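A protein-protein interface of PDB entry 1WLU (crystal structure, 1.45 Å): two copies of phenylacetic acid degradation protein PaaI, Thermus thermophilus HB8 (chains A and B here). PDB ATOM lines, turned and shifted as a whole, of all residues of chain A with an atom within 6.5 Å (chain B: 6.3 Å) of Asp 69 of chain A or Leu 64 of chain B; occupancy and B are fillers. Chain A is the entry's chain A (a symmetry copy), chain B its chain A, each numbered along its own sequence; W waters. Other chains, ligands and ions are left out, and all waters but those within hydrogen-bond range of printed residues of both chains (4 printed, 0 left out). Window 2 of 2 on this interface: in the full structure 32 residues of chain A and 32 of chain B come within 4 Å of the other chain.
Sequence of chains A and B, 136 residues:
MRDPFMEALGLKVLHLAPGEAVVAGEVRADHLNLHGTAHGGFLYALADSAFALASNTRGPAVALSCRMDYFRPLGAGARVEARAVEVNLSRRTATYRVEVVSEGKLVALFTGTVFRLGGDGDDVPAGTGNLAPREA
O of Leu 64 of chain B lies within hydrogen-bond range of N of Tyr 70 of chain A (2.9 Å).
The backbone NH (N) of Met 68 of chain A is in hydrogen-bond range of the backbone carbonyl oxygen (O) of Cys 66 of chain B (2.8 Å).
The side-chain carboxylate (OD1) of Asp 69 of chain A lies within hydrogen-bond range of the side-chain hydroxyl (OG) of Ser 65 of chain B (2.7 Å).
OG of Ser 65 of chain B lies close to NH2 of Arg 67 of chain A (3.2 Å).
O of Ser 65 of chain B sits at hydrogen-bond distance from N of Thr 113 of chain B (2.9 Å).
NE of Arg 67 of chain A is in salt-bridge range of OD2 of Asp 69 of chain A (2.9 Å).
The backbone NH of Asp 69 of chain A lies within hydrogen-bond range of the backbone carbonyl oxygen of Leu 109 of chain A (2.8 Å).
O of Thr 111 of chain A lies within hydrogen-bond range of N of Arg 67 of chain A (2.7 Å).
N of Leu 64 of chain B sits at hydrogen-bond distance from O of Thr 113 of chain B (2.8 Å).
Among the printed residues, merely in contact across the chains: Arg 67 of chain A with Cys 66 of chain B, Met 68 of chain A with Leu 64 of chain B, Met 68 of chain A with Ser 65 of chain B, Asp 69 of chain A with Leu 64 of chain B and Tyr 70 of chain A with Ala 63 of chain B.
Of the printed residues of chain B, Arg 67 of chain A touches Ser 65 and Cys 66.
Of the printed residues of chain B, Met 68 of chain A touches Leu 64, Ser 65 and Cys 66.
Asp 69 of chain A touches just these residues of chain B: Leu 64 and Ser 65.
Printed residues of chain A within 4 Å of Ala 63 of chain B: Tyr 70.
Printed residues of chain A within 4 Å of Ser 65 of chain B: Arg 67, Met 68 and Asp 69.
Of the printed residues of chain A, Cys 66 of chain B touches Arg 67 (3.2 Å) and Met 68 (2.8 Å).
Phe 115 of chain B touches none of the printed residues of chain A.
The nearest residue of chain A that does not touch Leu 64 of chain B is Phe 71 of chain A (5.7 Å).
Hydrophobic or aromatic side chains of chain B that line the printed part of chain A: Ala 63.
Printed residues of chain A that touch a printed residue of chain B: Arg 67, Met 68, Asp 69 and Tyr 70.
Among the printed residues, 9 pairs touch across the chains.
Among the printed residues, no Asp or Glu carboxylate lies within 4 Å of a Lys or Arg side-chain nitrogen of the other chain.
No position is printed for both chains.
Water W4 bridges OD1 of Asp 69 of chain A and O of Leu 64 of chain B.
Water W3 lies within hydrogen-bond range of the backbone carbonyl oxygen of Tyr 70 of chain A (2.8 Å) and the backbone carbonyl oxygen of Leu 64 of chain B (3.2 Å).
Water W1 lies within hydrogen-bond range of the backbone carbonyl oxygen of Ala 63 of chain B (2.8 Å) and the backbone carbonyl oxygen of Tyr 70 of chain A (2.8 Å).
Water W2 lies within hydrogen-bond range of OH of Tyr 70 of chain A (3.0 Å) and SG of Cys 66 of chain B (3.4 Å).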
ATOM      1  N   ARG A  67      27.742  16.495  -2.196  1.00  0.00           N
ATOM      2  CA  ARG A  67      27.908  17.322  -3.383  1.00  0.00           C
ATOM      3  C   ARG A  67      27.155  18.622  -3.165  1.00  0.00           C
ATOM      4  O   ARG A  67      26.035  18.627  -2.646  1.00  0.00           O
ATOM      5  CB  ARG A  67      27.350  16.612  -4.619  1.00  0.00           C
ATOM      6  CG  ARG A  67      27.400  17.438  -5.907  1.00  0.00           C
ATOM      7  CD  ARG A  67      26.729  16.660  -7.030  1.00  0.00           C
ATOM      8  NE  ARG A  67      26.599  17.416  -8.275  1.00  0.00           N
ATOM      9  CZ  ARG A  67      27.344  17.229  -9.360  1.00  0.00           C
ATOM     10  NH1 ARG A  67      28.299  16.306  -9.378  1.00  0.00           N
ATOM     11  NH2 ARG A  67      27.114  17.955 -10.446  1.00  0.00           N
ATOM     12  N   MET A  68      27.780  19.725  -3.553  1.00  0.00           N
ATOM     13  CA  MET A  68      27.170  21.035  -3.417  1.00  0.00           C
ATOM     14  C   MET A  68      27.212  21.727  -4.776  1.00  0.00           C
ATOM     15  O   MET A  68      28.293  21.950  -5.330  1.00  0.00           O
ATOM     16  CB  MET A  68      27.936  21.866  -2.384  1.00  0.00           C
ATOM     17  CG  MET A  68      27.333  23.226  -2.102  1.00  0.00           C
ATOM     18  SD  MET A  68      25.806  23.128  -1.156  1.00  0.00           S
ATOM     19  CE  MET A  68      25.675  24.834  -0.597  1.00  0.00           C
ATOM     20  N   ASP A  69      26.037  22.037  -5.316  1.00  0.00           N
ATOM     21  CA  ASP A  69      25.923  22.721  -6.600  1.00  0.00           C
ATOM     22  C   ASP A  69      25.425  24.134  -6.322  1.00  0.00           C
ATOM     23  O   ASP A  69      24.356  24.320  -5.745  1.00  0.00           O
ATOM     24  CB  ASP A  69      24.951  21.971  -7.517  1.00  0.00           C
ATOM     25  CG  ASP A  69      25.496  20.626  -7.966  1.00  0.00           C
ATOM     26  OD1 ASP A  69      26.631  20.590  -8.486  1.00  0.00           O
ATOM     27  OD2 ASP A  69      24.790  19.607  -7.809  1.00  0.00           O
ATOM     28  N   TYR A  70      26.214  25.123  -6.731  1.00  0.00           N
ATOM     29  CA  TYR A  70      25.895  26.533  -6.501  1.00  0.00           C
ATOM     30  C   TYR A  70      25.235  27.179  -7.710  1.00  0.00           C
ATOM     31  O   TYR A  70      25.757  27.095  -8.823  1.00  0.00           O
ATOM     32  CB  TYR A  70      27.181  27.288  -6.162  1.00  0.00           C
ATOM     33  CG  TYR A  70      27.859  26.811  -4.900  1.00  0.00           C
ATOM     34  CD1 TYR A  70      27.557  27.377  -3.664  1.00  0.00           C
ATOM     35  CD2 TYR A  70      28.810  25.794  -4.941  1.00  0.00           C
ATOM     36  CE1 TYR A  70      28.187  26.947  -2.501  1.00  0.00           C
ATOM     37  CE2 TYR A  70      29.444  25.354  -3.784  1.00  0.00           C
ATOM     38  CZ  TYR A  70      29.128  25.937  -2.568  1.00  0.00           C
ATOM     39  OH  TYR A  70      29.756  25.524  -1.419  1.00  0.00           O
ATOM     40  N   PHE A  71      24.101  27.846  -7.489  1.00  0.00           N
ATOM     41  CA  PHE A  71      23.379  28.482  -8.593  1.00  0.00           C
ATOM     42  C   PHE A  71      23.344  30.004  -8.570  1.00  0.00           C
ATOM     43  O   PHE A  71      23.428  30.641  -9.621  1.00  0.00           O
ATOM     44  CB  PHE A  71      21.930  27.985  -8.652  1.00  0.00           C
ATOM     45  CG  PHE A  71      21.792  26.491  -8.624  1.00  0.00           C
ATOM     46  CD1 PHE A  71      22.564  25.686  -9.455  1.00  0.00           C
ATOM     47  CD2 PHE A  71      20.874  25.888  -7.771  1.00  0.00           C
ATOM     48  CE1 PHE A  71      22.424  24.298  -9.437  1.00  0.00           C
ATOM     49  CE2 PHE A  71      20.727  24.504  -7.746  1.00  0.00           C
ATOM     50  CZ  PHE A  71      21.503  23.707  -8.579  1.00  0.00           C
ATOM     51  N   VAL A 107      19.097  28.707  -4.323  1.00  0.00           N
ATOM     52  CA  VAL A 107      20.467  29.207  -4.350  1.00  0.00           C
ATOM     53  C   VAL A 107      21.505  28.110  -4.578  1.00  0.00           C
ATOM     54  O   VAL A 107      22.546  28.345  -5.197  1.00  0.00           O
ATOM     55  CB  VAL A 107      20.786  29.938  -3.020  1.00  0.00           C
ATOM     56  CG1 VAL A 107      22.247  30.353  -2.970  1.00  0.00           C
ATOM     57  CG2 VAL A 107      19.885  31.156  -2.877  1.00  0.00           C
ATOM     58  N   ALA A 108      21.220  26.914  -4.074  1.00  0.00           N
ATOM     59  CA  ALA A 108      22.138  25.789  -4.215  1.00  0.00           C
ATOM     60  C   ALA A 108      21.421  24.482  -3.927  1.00  0.00           C
ATOM     61  O   ALA A 108      20.346  24.470  -3.326  1.00  0.00           O
ATOM     62  CB  ALA A 108      23.324  25.952  -3.260  1.00  0.00           C
ATOM     63  N   LEU A 109      22.025  23.386  -4.372  1.00  0.00           N
ATOM     64  CA  LEU A 109      21.479  22.052  -4.159  1.00  0.00           C
ATOM     65  C   LEU A 109      22.578  21.185  -3.563  1.00  0.00           C
ATOM     66  O   LEU A 109      23.674  21.084  -4.117  1.00  0.00           O
ATOM     67  CB  LEU A 109      21.014  21.439  -5.481  1.00  0.00           C
ATOM     68  CG  LEU A 109      20.498  19.999  -5.384  1.00  0.00           C
ATOM     69  CD1 LEU A 109      19.202  19.974  -4.590  1.00  0.00           C
ATOM     70  CD2 LEU A 109      20.275  19.436  -6.780  1.00  0.00           C
ATOM     71  N   PHE A 110      22.270  20.556  -2.436  1.00  0.00           N
ATOM     72  CA  PHE A 110      23.207  19.693  -1.728  1.00  0.00           C
ATOM     73  C   PHE A 110      22.662  18.268  -1.764  1.00  0.00           C
ATOM     74  O   PHE A 110      21.471  18.041  -1.565  1.00  0.00           O
ATOM     75  CB  PHE A 110      23.347  20.230  -0.290  1.00  0.00           C
ATOM     76  CG  PHE A 110      24.131  19.349   0.651  1.00  0.00           C
ATOM     77  CD1 PHE A 110      23.606  18.141   1.107  1.00  0.00           C
ATOM     78  CD2 PHE A 110      25.354  19.782   1.162  1.00  0.00           C
ATOM     79  CE1 PHE A 110      24.284  17.384   2.065  1.00  0.00           C
ATOM     80  CE2 PHE A 110      26.036  19.031   2.119  1.00  0.00           C
ATOM     81  CZ  PHE A 110      25.497  17.833   2.571  1.00  0.00           C
ATOM     82  N   THR A 111      23.539  17.317  -2.056  1.00  0.00           N
ATOM     83  CA  THR A 111      23.169  15.909  -2.112  1.00  0.00           C
ATOM     84  C   THR A 111      24.195  15.188  -1.248  1.00  0.00           C
ATOM     85  O   THR A 111      25.392  15.285  -1.503  1.00  0.00           O
ATOM     86  CB  THR A 111      23.251  15.372  -3.556  1.00  0.00           C
ATOM     87  OG1 THR A 111      22.536  16.249  -4.436  1.00  0.00           O
ATOM     88  CG2 THR A 111      22.641  13.976  -3.638  1.00  0.00           C
ATOM     89  N   PHE B  51      40.613  25.892  -2.668  1.00  0.00           N
ATOM     90  CA  PHE B  51      40.025  25.747  -4.000  1.00  0.00           C
ATOM     91  C   PHE B  51      39.810  27.132  -4.621  1.00  0.00           C
ATOM     92  O   PHE B  51      40.162  27.371  -5.779  1.00  0.00           O
ATOM     93  CB  PHE B  51      38.696  24.989  -3.831  1.00  0.00           C
ATOM     94  CG  PHE B  51      37.781  25.023  -5.026  1.00  0.00           C
ATOM     95  CD1 PHE B  51      38.154  24.455  -6.239  1.00  0.00           C
ATOM     96  CD2 PHE B  51      36.495  25.536  -4.896  1.00  0.00           C
ATOM     97  CE1 PHE B  51      37.252  24.388  -7.298  1.00  0.00           C
ATOM     98  CE2 PHE B  51      35.586  25.474  -5.951  1.00  0.00           C
ATOM     99  CZ  PHE B  51      35.968  24.896  -7.152  1.00  0.00           C
ATOM    100  N   VAL B  62      34.065  31.278 -10.084  1.00  0.00           N
ATOM    101  CA  VAL B  62      33.126  30.940  -9.024  1.00  0.00           C
ATOM    102  C   VAL B  62      32.795  29.458  -9.106  1.00  0.00           C
ATOM    103  O   VAL B  62      32.742  28.876 -10.191  1.00  0.00           O
ATOM    104  CB  VAL B  62      31.822  31.762  -9.129  1.00  0.00           C
ATOM    105  CG1 VAL B  62      32.120  33.237  -8.882  1.00  0.00           C
ATOM    106  CG2 VAL B  62      31.186  31.565 -10.493  1.00  0.00           C
ATOM    107  N   ALA B  63      32.571  28.851  -7.949  1.00  0.00           N
ATOM    108  CA  ALA B  63      32.265  27.432  -7.891  1.00  0.00           C
ATOM    109  C   ALA B  63      30.953  27.055  -8.556  1.00  0.00           C
ATOM    110  O   ALA B  63      29.962  27.781  -8.466  1.00  0.00           O
ATOM    111  CB  ALA B  63      32.244  26.970  -6.443  1.00  0.00           C
ATOM    112  N   LEU B  64      30.969  25.915  -9.238  1.00  0.00           N
ATOM    113  CA  LEU B  64      29.779  25.368  -9.870  1.00  0.00           C
ATOM    114  C   LEU B  64      29.368  24.144  -9.055  1.00  0.00           C
ATOM    115  O   LEU B  64      28.313  24.138  -8.426  1.00  0.00           O
ATOM    116  CB  LEU B  64      30.057  24.949 -11.319  1.00  0.00           C
ATOM    117  CG  LEU B  64      30.196  26.059 -12.366  1.00  0.00           C
ATOM    118  CD1 LEU B  64      30.545  25.440 -13.710  1.00  0.00           C
ATOM    119  CD2 LEU B  64      28.899  26.853 -12.463  1.00  0.00           C
ATOM    120  N   SER B  65      30.222  23.123  -9.051  1.00  0.00           N
ATOM    121  CA  SER B  65      29.945  21.883  -8.330  1.00  0.00           C
ATOM    122  C   SER B  65      31.155  21.390  -7.552  1.00  0.00           C
ATOM    123  O   SER B  65      32.261  21.331  -8.087  1.00  0.00           O
ATOM    124  CB  SER B  65      29.519  20.795  -9.315  1.00  0.00           C
ATOM    125  OG  SER B  65      29.186  19.601  -8.628  1.00  0.00           O
ATOM    126  N   CYS B  66      30.931  21.022  -6.294  1.00  0.00           N
ATOM    127  CA  CYS B  66      32.002  20.525  -5.440  1.00  0.00           C
ATOM    128  C   CYS B  66      31.579  19.266  -4.705  1.00  0.00           C
ATOM    129  O   CYS B  66      30.432  19.140  -4.272  1.00  0.00           O
ATOM    130  CB  CYS B  66      32.397  21.588  -4.417  1.00  0.00           C
ATOM    131  SG  CYS B  66      32.892  23.149  -5.167  1.00  0.00           S
ATOM    132  N   ARG B  92      36.381  28.164 -20.214  1.00  0.00           N
ATOM    133  CA  ARG B  92      35.344  28.684 -19.326  1.00  0.00           C
ATOM    134  C   ARG B  92      35.126  27.923 -18.022  1.00  0.00           C
ATOM    135  O   ARG B  92      34.284  28.313 -17.213  1.00  0.00           O
ATOM    136  CB  ARG B  92      34.010  28.782 -20.077  1.00  0.00           C
ATOM    137  CG  ARG B  92      34.047  29.681 -21.311  1.00  0.00           C
ATOM    138  CD  ARG B  92      34.702  31.027 -21.015  1.00  0.00           C
ATOM    139  NE  ARG B  92      34.023  31.774 -19.958  1.00  0.00           N
ATOM    140  CZ  ARG B  92      32.821  32.328 -20.082  1.00  0.00           C
ATOM    141  NH1 ARG B  92      32.150  32.220 -21.221  1.00  0.00           N
ATOM    142  NH2 ARG B  92      32.292  32.996 -19.066  1.00  0.00           N
ATOM    143  N   THR B  93      35.877  26.846 -17.816  1.00  0.00           N
ATOM    144  CA  THR B  93      35.754  26.059 -16.591  1.00  0.00           C
ATOM    145  C   THR B  93      37.112  25.493 -16.200  1.00  0.00           C
ATOM    146  O   THR B  93      38.022  25.418 -17.022  1.00  0.00           O
ATOM    147  CB  THR B  93      34.769  24.876 -16.760  1.00  0.00           C
ATOM    148  OG1 THR B  93      35.200  24.046 -17.844  1.00  0.00           O
ATOM    149  CG2 THR B  93      33.356  25.380 -17.030  1.00  0.00           C
ATOM    150  N   THR B 113      34.740  22.107  -9.403  1.00  0.00           N
ATOM    151  CA  THR B 113      34.823  22.727 -10.715  1.00  0.00           C
ATOM    152  C   THR B 113      34.274  24.141 -10.639  1.00  0.00           C
ATOM    153  O   THR B 113      33.237  24.384 -10.020  1.00  0.00           O
ATOM    154  CB  THR B 113      34.024  21.923 -11.751  1.00  0.00           C
ATOM    155  OG1 THR B 113      34.660  20.655 -11.944  1.00  0.00           O
ATOM    156  CG2 THR B 113      33.959  22.665 -13.083  1.00  0.00           C
ATOM    157  N   VAL B 114      34.988  25.072 -11.261  1.00  0.00           N
ATOM    158  CA  VAL B 114      34.578  26.469 -11.280  1.00  0.00           C
ATOM    159  C   VAL B 114      34.195  26.908 -12.679  1.00  0.00           C
ATOM    160  O   VAL B 114      34.534  26.260 -13.674  1.00  0.00           O
ATOM    161  CB  VAL B 114      35.712  27.434 -10.834  1.00  0.00           C
ATOM    162  CG1 VAL B 114      36.084  27.193  -9.393  1.00  0.00           C
ATOM    163  CG2 VAL B 114      36.927  27.270 -11.746  1.00  0.00           C
ATOM    164  N   PHE B 115      33.479  28.024 -12.732  1.00  0.00           N
ATOM    165  CA  PHE B 115      33.088  28.643 -13.983  1.00  0.00           C
ATOM    166  C   PHE B 115      33.989  29.873 -14.031  1.00  0.00           C
ATOM    167  O   PHE B 115      34.049  30.638 -13.066  1.00  0.00           O
ATOM    168  CB  PHE B 115      31.617  29.060 -13.945  1.00  0.00           C
ATOM    169  CG  PHE B 115      31.167  29.795 -15.176  1.00  0.00           C
ATOM    170  CD1 PHE B 115      31.151  31.186 -15.206  1.00  0.00           C
ATOM    171  CD2 PHE B 115      30.780  29.096 -16.314  1.00  0.00           C
ATOM    172  CE1 PHE B 115      30.754  31.870 -16.355  1.00  0.00           C
ATOM    173  CE2 PHE B 115      30.382  29.770 -17.467  1.00  0.00           C
ATOM    174  CZ  PHE B 115      30.369  31.159 -17.486  1.00  0.00           C
HETATM  175  O   HOH W   1      27.702  28.980  -9.607  1.00  0.00           O
HETATM  176  O   HOH W   2      32.230  25.768  -3.063  1.00  0.00           O
HETATM  177  O   HOH W   3      26.256  25.078 -10.671  1.00  0.00           O
HETATM  178  O   HOH W   4      26.822  22.356 -10.610  1.00  0.00           O
